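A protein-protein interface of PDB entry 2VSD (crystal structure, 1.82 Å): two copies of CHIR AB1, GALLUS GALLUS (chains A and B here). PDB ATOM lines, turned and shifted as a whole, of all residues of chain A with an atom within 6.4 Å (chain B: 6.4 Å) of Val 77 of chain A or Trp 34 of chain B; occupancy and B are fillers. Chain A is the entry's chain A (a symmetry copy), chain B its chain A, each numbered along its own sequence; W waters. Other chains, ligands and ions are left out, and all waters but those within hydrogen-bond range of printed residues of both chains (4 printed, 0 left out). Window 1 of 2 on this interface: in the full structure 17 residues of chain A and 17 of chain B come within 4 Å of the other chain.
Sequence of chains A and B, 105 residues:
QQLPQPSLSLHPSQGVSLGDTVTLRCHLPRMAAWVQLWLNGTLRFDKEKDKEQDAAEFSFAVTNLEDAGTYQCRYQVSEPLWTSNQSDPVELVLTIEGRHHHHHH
Ser 78 of chain B touches Ala 32 of chain A (O to CB, 3.6 Å).
CE3 of Trp 34 of chain B touches NE2 of Gln 76 of chain A (3.5 Å).
Ala 32 of chain B touches Ser 78 of chain A.
Ser 78 of chain A touches Val 77 of chain B.
Ala 32 of chain B touches Glu 79 of chain A.
Ala 32 of chain B touches Leu 81 of chain A.
Ala 33 of chain B touches Leu 81 of chain A.
CD2 of Leu 81 of chain A touches CD1 of Trp 34 of chain B (3.8 Å).
Leu 81 of chain A touches Lys 49 of chain B.
CZ2 of Trp 34 of chain B touches CB of Thr 83 of chain A, 3.7 Å away.
Of the 15 printed residues of chain B, 8 touch a printed residue of chain A.
Hydrophobic or aromatic side chains of chain B within 4 Å of the printed part of chain A: Ala 32, Trp 34 and Val 77.
Along chain B the printed residues that touch a printed residue of chain A span positions 32 to 78.
Printed residues of chain A that touch a printed residue of chain B: Ala 32, Trp 34, Arg 74, Gln 76, Val 77, Ser 78, Glu 79, Leu 81, Trp 82 and Thr 83.
Hydrophobic or aromatic side chains of chain A within 4 Å of the printed part of chain B: Ala 32, Trp 34, Val 77 and Leu 81.
Along chain A the printed residues that touch a printed residue of chain B span positions 32 to 83.
Among the printed residues, 18 pairs touch across the chains.
Among the printed residues, Asp or Glu carboxylates within 4 Å of a Lys or Arg side-chain nitrogen of the other chain: Arg 74 of chain A with Asp 46 of chain B.
The backbone carbonyl oxygen (O) of Val 77 of chain A is in hydrogen-bond range of the indole nitrogen (NE1) of Trp 34 of chain B, 3.0 Å away.
The indole nitrogen of Trp 34 of chain B lies within hydrogen-bond range of the backbone carbonyl oxygen of Trp 82 of chain A, at 3.4 Å.
OD2 of Asp 46 of chain B lies within salt-bridge range of NH1 of Arg 74 of chain A, at 2.9 Å.
OD2 of Asp 46 of chain B lies within hydrogen-bond range of NE2 of Gln 76 of chain A, 3.2 Å away.
The backbone carbonyl oxygen (O) of Val 77 of chain B is in hydrogen-bond range of the indole nitrogen (NE1) of Trp 34 of chain A.
OG of Ser 78 of chain B lies within hydrogen-bond range of N of Ser 78 of chain A (2.8 Å).
Of the printed residues of chain B, Arg 74 of chain A touches Asp 46.
Of chain B, only Trp 34 (3.0 Å) and Ser 78 (3.3 Å) come within 4 Å of Val 77 of chain A.
Of chain A, only Gln 76 (3.5 Å), Val 77 (3.0 Å), Leu 81 (3.8 Å), Trp 82 (3.4 Å) and Thr 83 (3.7 Å) come within 4 Å of Trp 34 of chain B.
Of the printed residues of chain A, Asp 46 of chain B touches Arg 74 and Gln 76.
Printed residues of chain A within 4 Å of Val 77 of chain B: Trp 34 and Ser 78.
The nearest residue of chain B that does not touch Val 77 of chain A is Val 77 of chain B (6.0 Å).
The nearest residue of chain A that does not touch Trp 34 of chain B is Ser 78 of chain A (4.6 Å).
Water W3 lies within hydrogen-bond range of the side-chain amide oxygen (OE1) of Gln 76 of chain A (2.6 Å), the side-chain carboxylate (OD2) of Asp 46 of chain B (2.8 Å) and the side-chain amide nitrogen (NE2) of Gln 36 of chain B (2.8 Å).
Water W4 bridges O of Ala 32 of chain A (2.8 Å) and OG of Ser 78 of chain B (3.1 Å).
Water W2 lies within hydrogen-bond range of O of Ala 32 of chain B, OE2 of Glu 79 of chain A and OG of Ser 78 of chain A.
Water W1 lies within hydrogen-bond range of OE1 of Gln 76 of chain B and OE1 of Gln 76 of chain A.
The backbone NH of Gln 76 of chain B sits at hydrogen-bond distance from the backbone carbonyl oxygen of Trp 34 of chain B.
NH2 of Arg 74 of chain B lies close to NE2 of Gln 76 of chain B (3.5 Å).
The side-chain amide nitrogen (NE2) of Gln 76 of chain A lies close to the guanidinium group (NH2) of Arg 74 of chain A, at 3.5 Å.
The side-chain hydroxyl of Thr 83 of chain A is in hydrogen-bond range of the guanidinium group of Arg 74 of chain A, at 3.4 Å.
The side-chain amide nitrogen (NE2) of Gln 76 of chain A lies close to the side-chain hydroxyl (OG1) of Thr 83 of chain A (3.4 Å).
The backbone NH of Val 77 of chain A sits at hydrogen-bond distance from the backbone carbonyl oxygen of Trp 82 of chain A, 3.0 Å away.
Ala 32 of chain A touches Ser 78 of chain B, and with the chains exchanged Ser 78 of chain A touches Ala 32 of chain B.
Trp 34 of chain A touches Val 77 of chain B, and with the chains exchanged Val 77 of chain A touches Trp 34 of chain B.
Val 77 of chain A touches Ser 78 of chain B, and with the chains exchanged Ser 78 of chain A touches Val 77 of chain B.
Ser 78 of chain B touches its own counterpart, Ser 78 of chain A.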
ATOM      1  N   LEU A   3       9.378 -39.833  16.012  1.00  0.00           N
ATOM      2  CA  LEU A   3      10.352 -39.478  17.087  1.00  0.00           C
ATOM      3  C   LEU A   3       9.885 -39.966  18.485  1.00  0.00           C
ATOM      4  O   LEU A   3       9.001 -39.361  19.093  1.00  0.00           O
ATOM      5  CB  LEU A   3      10.635 -37.960  17.075  1.00  0.00           C
ATOM      6  CG  LEU A   3      12.044 -37.628  17.561  1.00  0.00           C
ATOM      7  CD1 LEU A   3      12.650 -36.365  16.976  1.00  0.00           C
ATOM      8  CD2 LEU A   3      11.968 -37.498  19.028  1.00  0.00           C
ATOM      9  N   MET A  31      20.743 -42.255  18.095  1.00  0.00           N
ATOM     10  CA  MET A  31      20.968 -41.279  17.026  1.00  0.00           C
ATOM     11  C   MET A  31      21.704 -40.086  17.630  1.00  0.00           C
ATOM     12  O   MET A  31      21.556 -39.815  18.815  1.00  0.00           O
ATOM     13  CB  MET A  31      19.636 -40.815  16.437  1.00  0.00           C
ATOM     14  CG  MET A  31      18.645 -40.256  17.464  1.00  0.00           C
ATOM     15  SD  MET A  31      17.072 -39.792  16.737  1.00  0.00           S
ATOM     16  CE  MET A  31      16.219 -41.370  16.616  1.00  0.00           C
ATOM     17  N   ALA A  32      22.502 -39.384  16.837  1.00  0.00           N
ATOM     18  CA  ALA A  32      23.111 -38.128  17.290  1.00  0.00           C
ATOM     19  C   ALA A  32      21.988 -37.108  17.532  1.00  0.00           C
ATOM     20  O   ALA A  32      21.061 -36.989  16.736  1.00  0.00           O
ATOM     21  CB  ALA A  32      24.135 -37.601  16.260  1.00  0.00           C
ATOM     22  N   ALA A  33      22.043 -36.399  18.650  1.00  0.00           N
ATOM     23  CA  ALA A  33      20.954 -35.467  18.974  1.00  0.00           C
ATOM     24  C   ALA A  33      21.376 -34.432  20.012  1.00  0.00           C
ATOM     25  O   ALA A  33      22.292 -34.661  20.802  1.00  0.00           O
ATOM     26  CB  ALA A  33      19.713 -36.224  19.440  1.00  0.00           C
ATOM     27  N   TRP A  34      20.726 -33.280  19.967  1.00  0.00           N
ATOM     28  CA  TRP A  34      20.856 -32.254  21.011  1.00  0.00           C
ATOM     29  C   TRP A  34      19.826 -32.589  22.068  1.00  0.00           C
ATOM     30  O   TRP A  34      18.676 -32.787  21.743  1.00  0.00           O
ATOM     31  CB  TRP A  34      20.618 -30.845  20.426  1.00  0.00           C
ATOM     32  CG  TRP A  34      21.884 -30.284  19.875  1.00  0.00           C
ATOM     33  CD1 TRP A  34      22.267 -30.234  18.551  1.00  0.00           C
ATOM     34  CD2 TRP A  34      22.974 -29.744  20.626  1.00  0.00           C
ATOM     35  NE1 TRP A  34      23.507 -29.663  18.446  1.00  0.00           N
ATOM     36  CE2 TRP A  34      23.981 -29.384  19.698  1.00  0.00           C
ATOM     37  CE3 TRP A  34      23.189 -29.500  21.985  1.00  0.00           C
ATOM     38  CZ2 TRP A  34      25.159 -28.787  20.086  1.00  0.00           C
ATOM     39  CZ3 TRP A  34      24.379 -28.922  22.375  1.00  0.00           C
ATOM     40  CH2 TRP A  34      25.351 -28.568  21.429  1.00  0.00           C
ATOM     41  N   ARG A  74      13.869 -33.349  26.456  1.00  0.00           N
ATOM     42  CA  ARG A  74      13.383 -33.207  25.087  1.00  0.00           C
ATOM     43  C   ARG A  74      14.622 -33.410  24.230  1.00  0.00           C
ATOM     44  O   ARG A  74      15.726 -33.024  24.632  1.00  0.00           O
ATOM     45  CB  ARG A  74      12.900 -31.758  24.946  1.00  0.00           C
ATOM     46  CG  ARG A  74      12.280 -31.340  23.684  1.00  0.00           C
ATOM     47  CD  ARG A  74      11.690 -29.996  23.949  1.00  0.00           C
ATOM     48  NE  ARG A  74      11.064 -29.399  22.782  1.00  0.00           N
ATOM     49  CZ  ARG A  74      11.477 -28.303  22.167  1.00  0.00           C
ATOM     50  NH1 ARG A  74      12.571 -27.646  22.552  1.00  0.00           N
ATOM     51  NH2 ARG A  74      10.794 -27.886  21.114  1.00  0.00           N
ATOM     52  N   TYR A  75      14.486 -33.987  23.042  1.00  0.00           N
ATOM     53  CA  TYR A  75      15.654 -34.047  22.140  1.00  0.00           C
ATOM     54  C   TYR A  75      15.274 -33.683  20.716  1.00  0.00           C
ATOM     55  O   TYR A  75      14.095 -33.728  20.378  1.00  0.00           O
ATOM     56  CB  TYR A  75      16.400 -35.387  22.211  1.00  0.00           C
ATOM     57  CG  TYR A  75      15.637 -36.571  21.676  1.00  0.00           C
ATOM     58  CD1 TYR A  75      14.706 -37.244  22.473  1.00  0.00           C
ATOM     59  CD2 TYR A  75      15.873 -37.052  20.385  1.00  0.00           C
ATOM     60  CE1 TYR A  75      13.995 -38.352  21.991  1.00  0.00           C
ATOM     61  CE2 TYR A  75      15.168 -38.160  19.886  1.00  0.00           C
ATOM     62  CZ  TYR A  75      14.226 -38.802  20.694  1.00  0.00           C
ATOM     63  OH  TYR A  75      13.514 -39.910  20.237  1.00  0.00           O
ATOM     64  N   GLN A  76      16.285 -33.265  19.945  1.00  0.00           N
ATOM     65  CA  GLN A  76      16.102 -32.678  18.620  1.00  0.00           C
ATOM     66  C   GLN A  76      17.208 -33.091  17.668  1.00  0.00           C
ATOM     67  O   GLN A  76      18.382 -33.223  18.042  1.00  0.00           O
ATOM     68  CB  GLN A  76      16.082 -31.133  18.683  1.00  0.00           C
ATOM     69  CG  GLN A  76      15.045 -30.517  19.595  1.00  0.00           C
ATOM     70  CD  GLN A  76      14.977 -28.998  19.447  1.00  0.00           C
ATOM     71  OE1 GLN A  76      16.011 -28.318  19.388  1.00  0.00           O
ATOM     72  NE2 GLN A  76      13.763 -28.470  19.380  1.00  0.00           N
ATOM     73  N   VAL A  77      16.809 -33.275  16.411  1.00  0.00           N
ATOM     74  CA  VAL A  77      17.746 -33.544  15.333  1.00  0.00           C
ATOM     75  C   VAL A  77      17.430 -32.604  14.165  1.00  0.00           C
ATOM     76  O   VAL A  77      16.317 -32.118  14.045  1.00  0.00           O
ATOM     77  CB  VAL A  77      17.671 -35.024  14.853  1.00  0.00           C
ATOM     78  CG1 VAL A  77      18.113 -35.955  15.967  1.00  0.00           C
ATOM     79  CG2 VAL A  77      16.264 -35.366  14.376  1.00  0.00           C
ATOM     80  N   SER A  78      18.415 -32.365  13.304  1.00  0.00           N
ATOM     81  CA  SER A  78      18.201 -31.451  12.166  1.00  0.00           C
ATOM     82  C   SER A  78      18.107 -32.153  10.804  1.00  0.00           C
ATOM     83  O   SER A  78      17.902 -31.494   9.779  1.00  0.00           O
ATOM     84  CB  SER A  78      19.277 -30.362  12.127  1.00  0.00           C
ATOM     85  OG  SER A  78      20.553 -30.932  12.092  1.00  0.00           O
ATOM     86  N   GLU A  79      18.258 -33.474  10.803  1.00  0.00           N
ATOM     87  CA  GLU A  79      18.163 -34.284   9.580  1.00  0.00           C
ATOM     88  C   GLU A  79      17.464 -35.591   9.942  1.00  0.00           C
ATOM     89  O   GLU A  79      18.131 -36.532  10.371  1.00  0.00           O
ATOM     90  CB  GLU A  79      19.563 -34.617   9.028  1.00  0.00           C
ATOM     91  CG  GLU A  79      20.576 -33.469   9.025  1.00  0.00           C
ATOM     92  CD  GLU A  79      20.792 -32.874   7.653  1.00  0.00           C
ATOM     93  OE1 GLU A  79      21.403 -33.564   6.799  1.00  0.00           O
ATOM     94  OE2 GLU A  79      20.369 -31.714   7.425  1.00  0.00           O
ATOM     95  N   PRO A  80      16.129 -35.652   9.807  1.00  0.00           N
ATOM     96  CA  PRO A  80      15.178 -34.594   9.432  1.00  0.00           C
ATOM     97  C   PRO A  80      14.978 -33.589  10.573  1.00  0.00           C
ATOM     98  O   PRO A  80      15.560 -33.786  11.642  1.00  0.00           O
ATOM     99  CB  PRO A  80      13.880 -35.353   9.181  1.00  0.00           C
ATOM    100  CG  PRO A  80      13.998 -36.599   9.981  1.00  0.00           C
ATOM    101  CD  PRO A  80      15.459 -36.940  10.060  1.00  0.00           C
ATOM    102  N   LEU A  81      14.149 -32.559  10.356  1.00  0.00           N
ATOM    103  CA  LEU A  81      13.982 -31.475  11.342  1.00  0.00           C
ATOM    104  C   LEU A  81      12.884 -31.792  12.319  1.00  0.00           C
ATOM    105  O   LEU A  81      11.725 -31.383  12.144  1.00  0.00           O
ATOM    106  CB  LEU A  81      13.741 -30.109  10.680  1.00  0.00           C
ATOM    107  CG  LEU A  81      14.994 -29.263  10.406  1.00  0.00           C
ATOM    108  CD1 LEU A  81      14.701 -28.210   9.356  1.00  0.00           C
ATOM    109  CD2 LEU A  81      15.540 -28.617  11.654  1.00  0.00           C
ATOM    110  N   TRP A  82      13.278 -32.522  13.361  1.00  0.00           N
ATOM    111  CA  TRP A  82      12.338 -33.155  14.258  1.00  0.00           C
ATOM    112  C   TRP A  82      12.700 -32.847  15.702  1.00  0.00           C
ATOM    113  O   TRP A  82      13.872 -32.782  16.053  1.00  0.00           O
ATOM    114  CB  TRP A  82      12.347 -34.680  14.050  1.00  0.00           C
ATOM    115  CG  TRP A  82      11.474 -35.176  12.880  1.00  0.00           C
ATOM    116  CD1 TRP A  82      10.618 -34.425  12.101  1.00  0.00           C
ATOM    117  CD2 TRP A  82      11.334 -36.536  12.425  1.00  0.00           C
ATOM    118  NE1 TRP A  82       9.991 -35.232  11.166  1.00  0.00           N
ATOM    119  CE2 TRP A  82      10.411 -36.527  11.341  1.00  0.00           C
ATOM    120  CE3 TRP A  82      11.915 -37.757  12.809  1.00  0.00           C
ATOM    121  CZ2 TRP A  82      10.044 -37.695  10.656  1.00  0.00           C
ATOM    122  CZ3 TRP A  82      11.557 -38.923  12.110  1.00  0.00           C
ATOM    123  CH2 TRP A  82      10.625 -38.879  11.049  1.00  0.00           C
ATOM    124  N   THR A  83      11.669 -32.689  16.517  1.00  0.00           N
ATOM    125  CA  THR A  83      11.832 -32.617  17.980  1.00  0.00           C
ATOM    126  C   THR A  83      10.929 -33.633  18.665  1.00  0.00           C
ATOM    127  O   THR A  83       9.830 -33.928  18.181  1.00  0.00           O
ATOM    128  CB  THR A  83      11.560 -31.187  18.537  1.00  0.00           C
ATOM    129  OG1 THR A  83      11.790 -31.181  19.956  1.00  0.00           O
ATOM    130  CG2 THR A  83      10.148 -30.738  18.265  1.00  0.00           C
ATOM    131  N   LEU B  28      20.852 -16.806   9.221  1.00  0.00           N
ATOM    132  CA  LEU B  28      21.909 -17.813   9.267  1.00  0.00           C
ATOM    133  C   LEU B  28      22.096 -18.489   7.906  1.00  0.00           C
ATOM    134  O   LEU B  28      21.364 -18.171   6.972  1.00  0.00           O
ATOM    135  CB  LEU B  28      21.720 -18.815  10.429  1.00  0.00           C
ATOM    136  CG  LEU B  28      20.497 -19.565  11.015  1.00  0.00           C
ATOM    137  CD1 LEU B  28      19.126 -18.896  10.843  1.00  0.00           C
ATOM    138  CD2 LEU B  28      20.442 -21.062  10.639  1.00  0.00           C
ATOM    139  N   ALA B  32      19.636 -26.783   7.042  1.00  0.00           N
ATOM    140  CA  ALA B  32      18.521 -27.104   7.940  1.00  0.00           C
ATOM    141  C   ALA B  32      19.010 -26.954   9.389  1.00  0.00           C
ATOM    142  O   ALA B  32      20.107 -27.386   9.733  1.00  0.00           O
ATOM    143  CB  ALA B  32      17.982 -28.529   7.676  1.00  0.00           C
ATOM    144  N   ALA B  33      18.220 -26.306  10.232  1.00  0.00           N
ATOM    145  CA  ALA B  33      18.672 -26.061  11.608  1.00  0.00           C
ATOM    146  C   ALA B  33      17.511 -25.731  12.543  1.00  0.00           C
ATOM    147  O   ALA B  33      16.462 -25.256  12.108  1.00  0.00           O
ATOM    148  CB  ALA B  33      19.725 -24.956  11.646  1.00  0.00           C
ATOM    149  N   TRP B  34      17.700 -26.032  13.817  1.00  0.00           N
ATOM    150  CA  TRP B  34      16.781 -25.601  14.880  1.00  0.00           C
ATOM    151  C   TRP B  34      17.250 -24.231  15.318  1.00  0.00           C
ATOM    152  O   TRP B  34      18.415 -24.060  15.604  1.00  0.00           O
ATOM    153  CB  TRP B  34      16.797 -26.601  16.057  1.00  0.00           C
ATOM    154  CG  TRP B  34      15.826 -27.706  15.821  1.00  0.00           C
ATOM    155  CD1 TRP B  34      16.107 -28.981  15.375  1.00  0.00           C
ATOM    156  CD2 TRP B  34      14.404 -27.634  15.953  1.00  0.00           C
ATOM    157  NE1 TRP B  34      14.947 -29.700  15.265  1.00  0.00           N
ATOM    158  CE2 TRP B  34      13.886 -28.896  15.578  1.00  0.00           C
ATOM    159  CE3 TRP B  34      13.519 -26.641  16.383  1.00  0.00           C
ATOM    160  CZ2 TRP B  34      12.542 -29.186  15.634  1.00  0.00           C
ATOM    161  CZ3 TRP B  34      12.170 -26.925  16.418  1.00  0.00           C
ATOM    162  CH2 TRP B  34      11.691 -28.189  16.048  1.00  0.00           C
ATOM    163  N   VAL B  35      16.347 -23.253  15.329  1.00  0.00           N
ATOM    164  CA  VAL B  35      16.756 -21.889  15.672  1.00  0.00           C
ATOM    165  C   VAL B  35      16.109 -21.527  17.004  1.00  0.00           C
ATOM    166  O   VAL B  35      14.941 -21.846  17.212  1.00  0.00           O
ATOM    167  CB  VAL B  35      16.335 -20.900  14.591  1.00  0.00           C
ATOM    168  CG1 VAL B  35      16.916 -19.517  14.877  1.00  0.00           C
ATOM    169  CG2 VAL B  35      16.797 -21.397  13.204  1.00  0.00           C
ATOM    170  N   GLN B  36      16.870 -20.892  17.895  1.00  0.00           N
ATOM    171  CA  GLN B  36      16.336 -20.510  19.205  1.00  0.00           C
ATOM    172  C   GLN B  36      16.303 -18.994  19.388  1.00  0.00           C
ATOM    173  O   GLN B  36      17.276 -18.309  19.027  1.00  0.00           O
ATOM    174  CB  GLN B  36      17.235 -21.065  20.279  1.00  0.00           C
ATOM    175  CG  GLN B  36      17.316 -22.589  20.243  1.00  0.00           C
ATOM    176  CD  GLN B  36      18.216 -23.180  21.300  1.00  0.00           C
ATOM    177  OE1 GLN B  36      19.101 -22.510  21.854  1.00  0.00           O
ATOM    178  NE2 GLN B  36      18.021 -24.485  21.569  1.00  0.00           N
ATOM    179  N   ASP B  46      11.654 -21.676  20.158  1.00  0.00           N
ATOM    180  CA  ASP B  46      12.504 -22.268  19.131  1.00  0.00           C
ATOM    181  C   ASP B  46      11.621 -22.666  17.973  1.00  0.00           C
ATOM    182  O   ASP B  46      10.393 -22.748  18.131  1.00  0.00           O
ATOM    183  CB  ASP B  46      13.371 -23.425  19.658  1.00  0.00           C
ATOM    184  CG  ASP B  46      12.565 -24.670  20.045  1.00  0.00           C
ATOM    185  OD1 ASP B  46      11.352 -24.728  19.823  1.00  0.00           O
ATOM    186  OD2 ASP B  46      13.181 -25.577  20.615  1.00  0.00           O
ATOM    187  N   LYS B  47      12.230 -22.855  16.808  1.00  0.00           N
ATOM    188  CA  LYS B  47      11.509 -23.352  15.634  1.00  0.00           C
ATOM    189  C   LYS B  47      12.467 -23.909  14.580  1.00  0.00           C
ATOM    190  O   LYS B  47      13.671 -23.638  14.595  1.00  0.00           O
ATOM    191  CB  LYS B  47      10.658 -22.243  15.021  1.00  0.00           C
ATOM    192  CG  LYS B  47      11.472 -21.115  14.413  1.00  0.00           C
ATOM    193  CD  LYS B  47      10.570 -19.958  13.985  1.00  0.00           C
ATOM    194  CE  LYS B  47       9.728 -20.317  12.797  1.00  0.00           C
ATOM    195  NZ  LYS B  47       8.712 -19.273  12.490  1.00  0.00           N
ATOM    196  N   GLU B  48      11.908 -24.677  13.656  1.00  0.00           N
ATOM    197  CA  GLU B  48      12.669 -25.256  12.554  1.00  0.00           C
ATOM    198  C   GLU B  48      12.935 -24.195  11.505  1.00  0.00           C
ATOM    199  O   GLU B  48      12.077 -23.361  11.240  1.00  0.00           O
ATOM    200  CB  GLU B  48      11.851 -26.373  11.886  1.00  0.00           C
ATOM    201  CG  GLU B  48      11.286 -27.413  12.825  1.00  0.00           C
ATOM    202  CD  GLU B  48       9.945 -27.035  13.476  1.00  0.00           C
ATOM    203  OE1 GLU B  48       9.650 -25.821  13.675  1.00  0.00           O
ATOM    204  OE2 GLU B  48       9.188 -27.986  13.826  1.00  0.00           O
ATOM    205  N   LYS B  49      14.106 -24.257  10.888  1.00  0.00           N
ATOM    206  CA  LYS B  49      14.362 -23.467   9.692  1.00  0.00           C
ATOM    207  C   LYS B  49      14.801 -24.405   8.580  1.00  0.00           C
ATOM    208  O   LYS B  49      15.926 -24.932   8.612  1.00  0.00           O
ATOM    209  CB  LYS B  49      15.432 -22.401   9.934  1.00  0.00           C
ATOM    210  CG  LYS B  49      15.655 -21.482   8.718  1.00  0.00           C
ATOM    211  CD  LYS B  49      17.023 -20.830   8.700  1.00  0.00           C
ATOM    212  CE  LYS B  49      18.112 -21.752   8.184  1.00  0.00           C
ATOM    213  NZ  LYS B  49      17.958 -22.096   6.730  1.00  0.00           N
ATOM    214  N   ARG B  74      20.387 -18.262  18.457  1.00  0.00           N
ATOM    215  CA  ARG B  74      21.377 -19.334  18.482  1.00  0.00           C
ATOM    216  C   ARG B  74      20.814 -20.381  17.533  1.00  0.00           C
ATOM    217  O   ARG B  74      19.592 -20.548  17.447  1.00  0.00           O
ATOM    218  CB  ARG B  74      21.377 -19.892  19.910  1.00  0.00           C
ATOM    219  CG  ARG B  74      22.340 -20.943  20.258  1.00  0.00           C
ATOM    220  CD  ARG B  74      22.274 -21.077  21.742  1.00  0.00           C
ATOM    221  NE  ARG B  74      23.141 -22.117  22.267  1.00  0.00           N
ATOM    222  CZ  ARG B  74      22.733 -23.223  22.869  1.00  0.00           C
ATOM    223  NH1 ARG B  74      21.440 -23.513  23.015  1.00  0.00           N
ATOM    224  NH2 ARG B  74      23.651 -24.075  23.294  1.00  0.00           N
ATOM    225  N   TYR B  75      21.661 -21.117  16.823  1.00  0.00           N
ATOM    226  CA  TYR B  75      21.132 -22.237  16.020  1.00  0.00           C
ATOM    227  C   TYR B  75      21.989 -23.481  16.172  1.00  0.00           C
ATOM    228  O   TYR B  75      23.134 -23.375  16.600  1.00  0.00           O
ATOM    229  CB  TYR B  75      20.913 -21.869  14.546  1.00  0.00           C
ATOM    230  CG  TYR B  75      22.169 -21.597  13.761  1.00  0.00           C
ATOM    231  CD1 TYR B  75      22.786 -20.343  13.804  1.00  0.00           C
ATOM    232  CD2 TYR B  75      22.726 -22.581  12.937  1.00  0.00           C
ATOM    233  CE1 TYR B  75      23.952 -20.075  13.073  1.00  0.00           C
ATOM    234  CE2 TYR B  75      23.895 -22.328  12.200  1.00  0.00           C
ATOM    235  CZ  TYR B  75      24.505 -21.073  12.277  1.00  0.00           C
ATOM    236  OH  TYR B  75      25.661 -20.784  11.551  1.00  0.00           O
ATOM    237  N   GLN B  76      21.376 -24.635  15.880  1.00  0.00           N
ATOM    238  CA  GLN B  76      21.953 -25.949  16.155  1.00  0.00           C
ATOM    239  C   GLN B  76      21.612 -26.948  15.066  1.00  0.00           C
ATOM    240  O   GLN B  76      20.511 -26.950  14.498  1.00  0.00           O
ATOM    241  CB  GLN B  76      21.445 -26.520  17.499  1.00  0.00           C
ATOM    242  CG  GLN B  76      21.683 -25.660  18.720  1.00  0.00           C
ATOM    243  CD  GLN B  76      21.321 -26.385  20.015  1.00  0.00           C
ATOM    244  OE1 GLN B  76      20.276 -27.044  20.105  1.00  0.00           O
ATOM    245  NE2 GLN B  76      22.187 -26.269  21.013  1.00  0.00           N
ATOM    246  N   VAL B  77      22.582 -27.819  14.798  1.00  0.00           N
ATOM    247  CA  VAL B  77      22.392 -28.932  13.882  1.00  0.00           C
ATOM    248  C   VAL B  77      22.893 -30.212  14.557  1.00  0.00           C
ATOM    249  O   VAL B  77      23.713 -30.156  15.459  1.00  0.00           O
ATOM    250  CB  VAL B  77      23.151 -28.713  12.539  1.00  0.00           C
ATOM    251  CG1 VAL B  77      22.568 -27.522  11.800  1.00  0.00           C
ATOM    252  CG2 VAL B  77      24.644 -28.530  12.785  1.00  0.00           C
ATOM    253  N   SER B  78      22.401 -31.361  14.103  1.00  0.00           N
ATOM    254  CA  SER B  78      22.812 -32.638  14.716  1.00  0.00           C
ATOM    255  C   SER B  78      23.744 -33.486  13.839  1.00  0.00           C
ATOM    256  O   SER B  78      24.177 -34.565  14.256  1.00  0.00           O
ATOM    257  CB  SER B  78      21.591 -33.462  15.140  1.00  0.00           C
ATOM    258  OG  SER B  78      20.736 -33.667  14.053  1.00  0.00           O
HETATM  259  O   HOH W   1      18.676 -28.663  18.329  1.00  0.00           O
HETATM  260  O   HOH W   2      21.485 -29.849   9.355  1.00  0.00           O
HETATM  261  O   HOH W   3      15.907 -25.839  20.251  1.00  0.00           O
HETATM  262  O   HOH W   4      20.885 -36.747  13.905  1.00  0.00           O
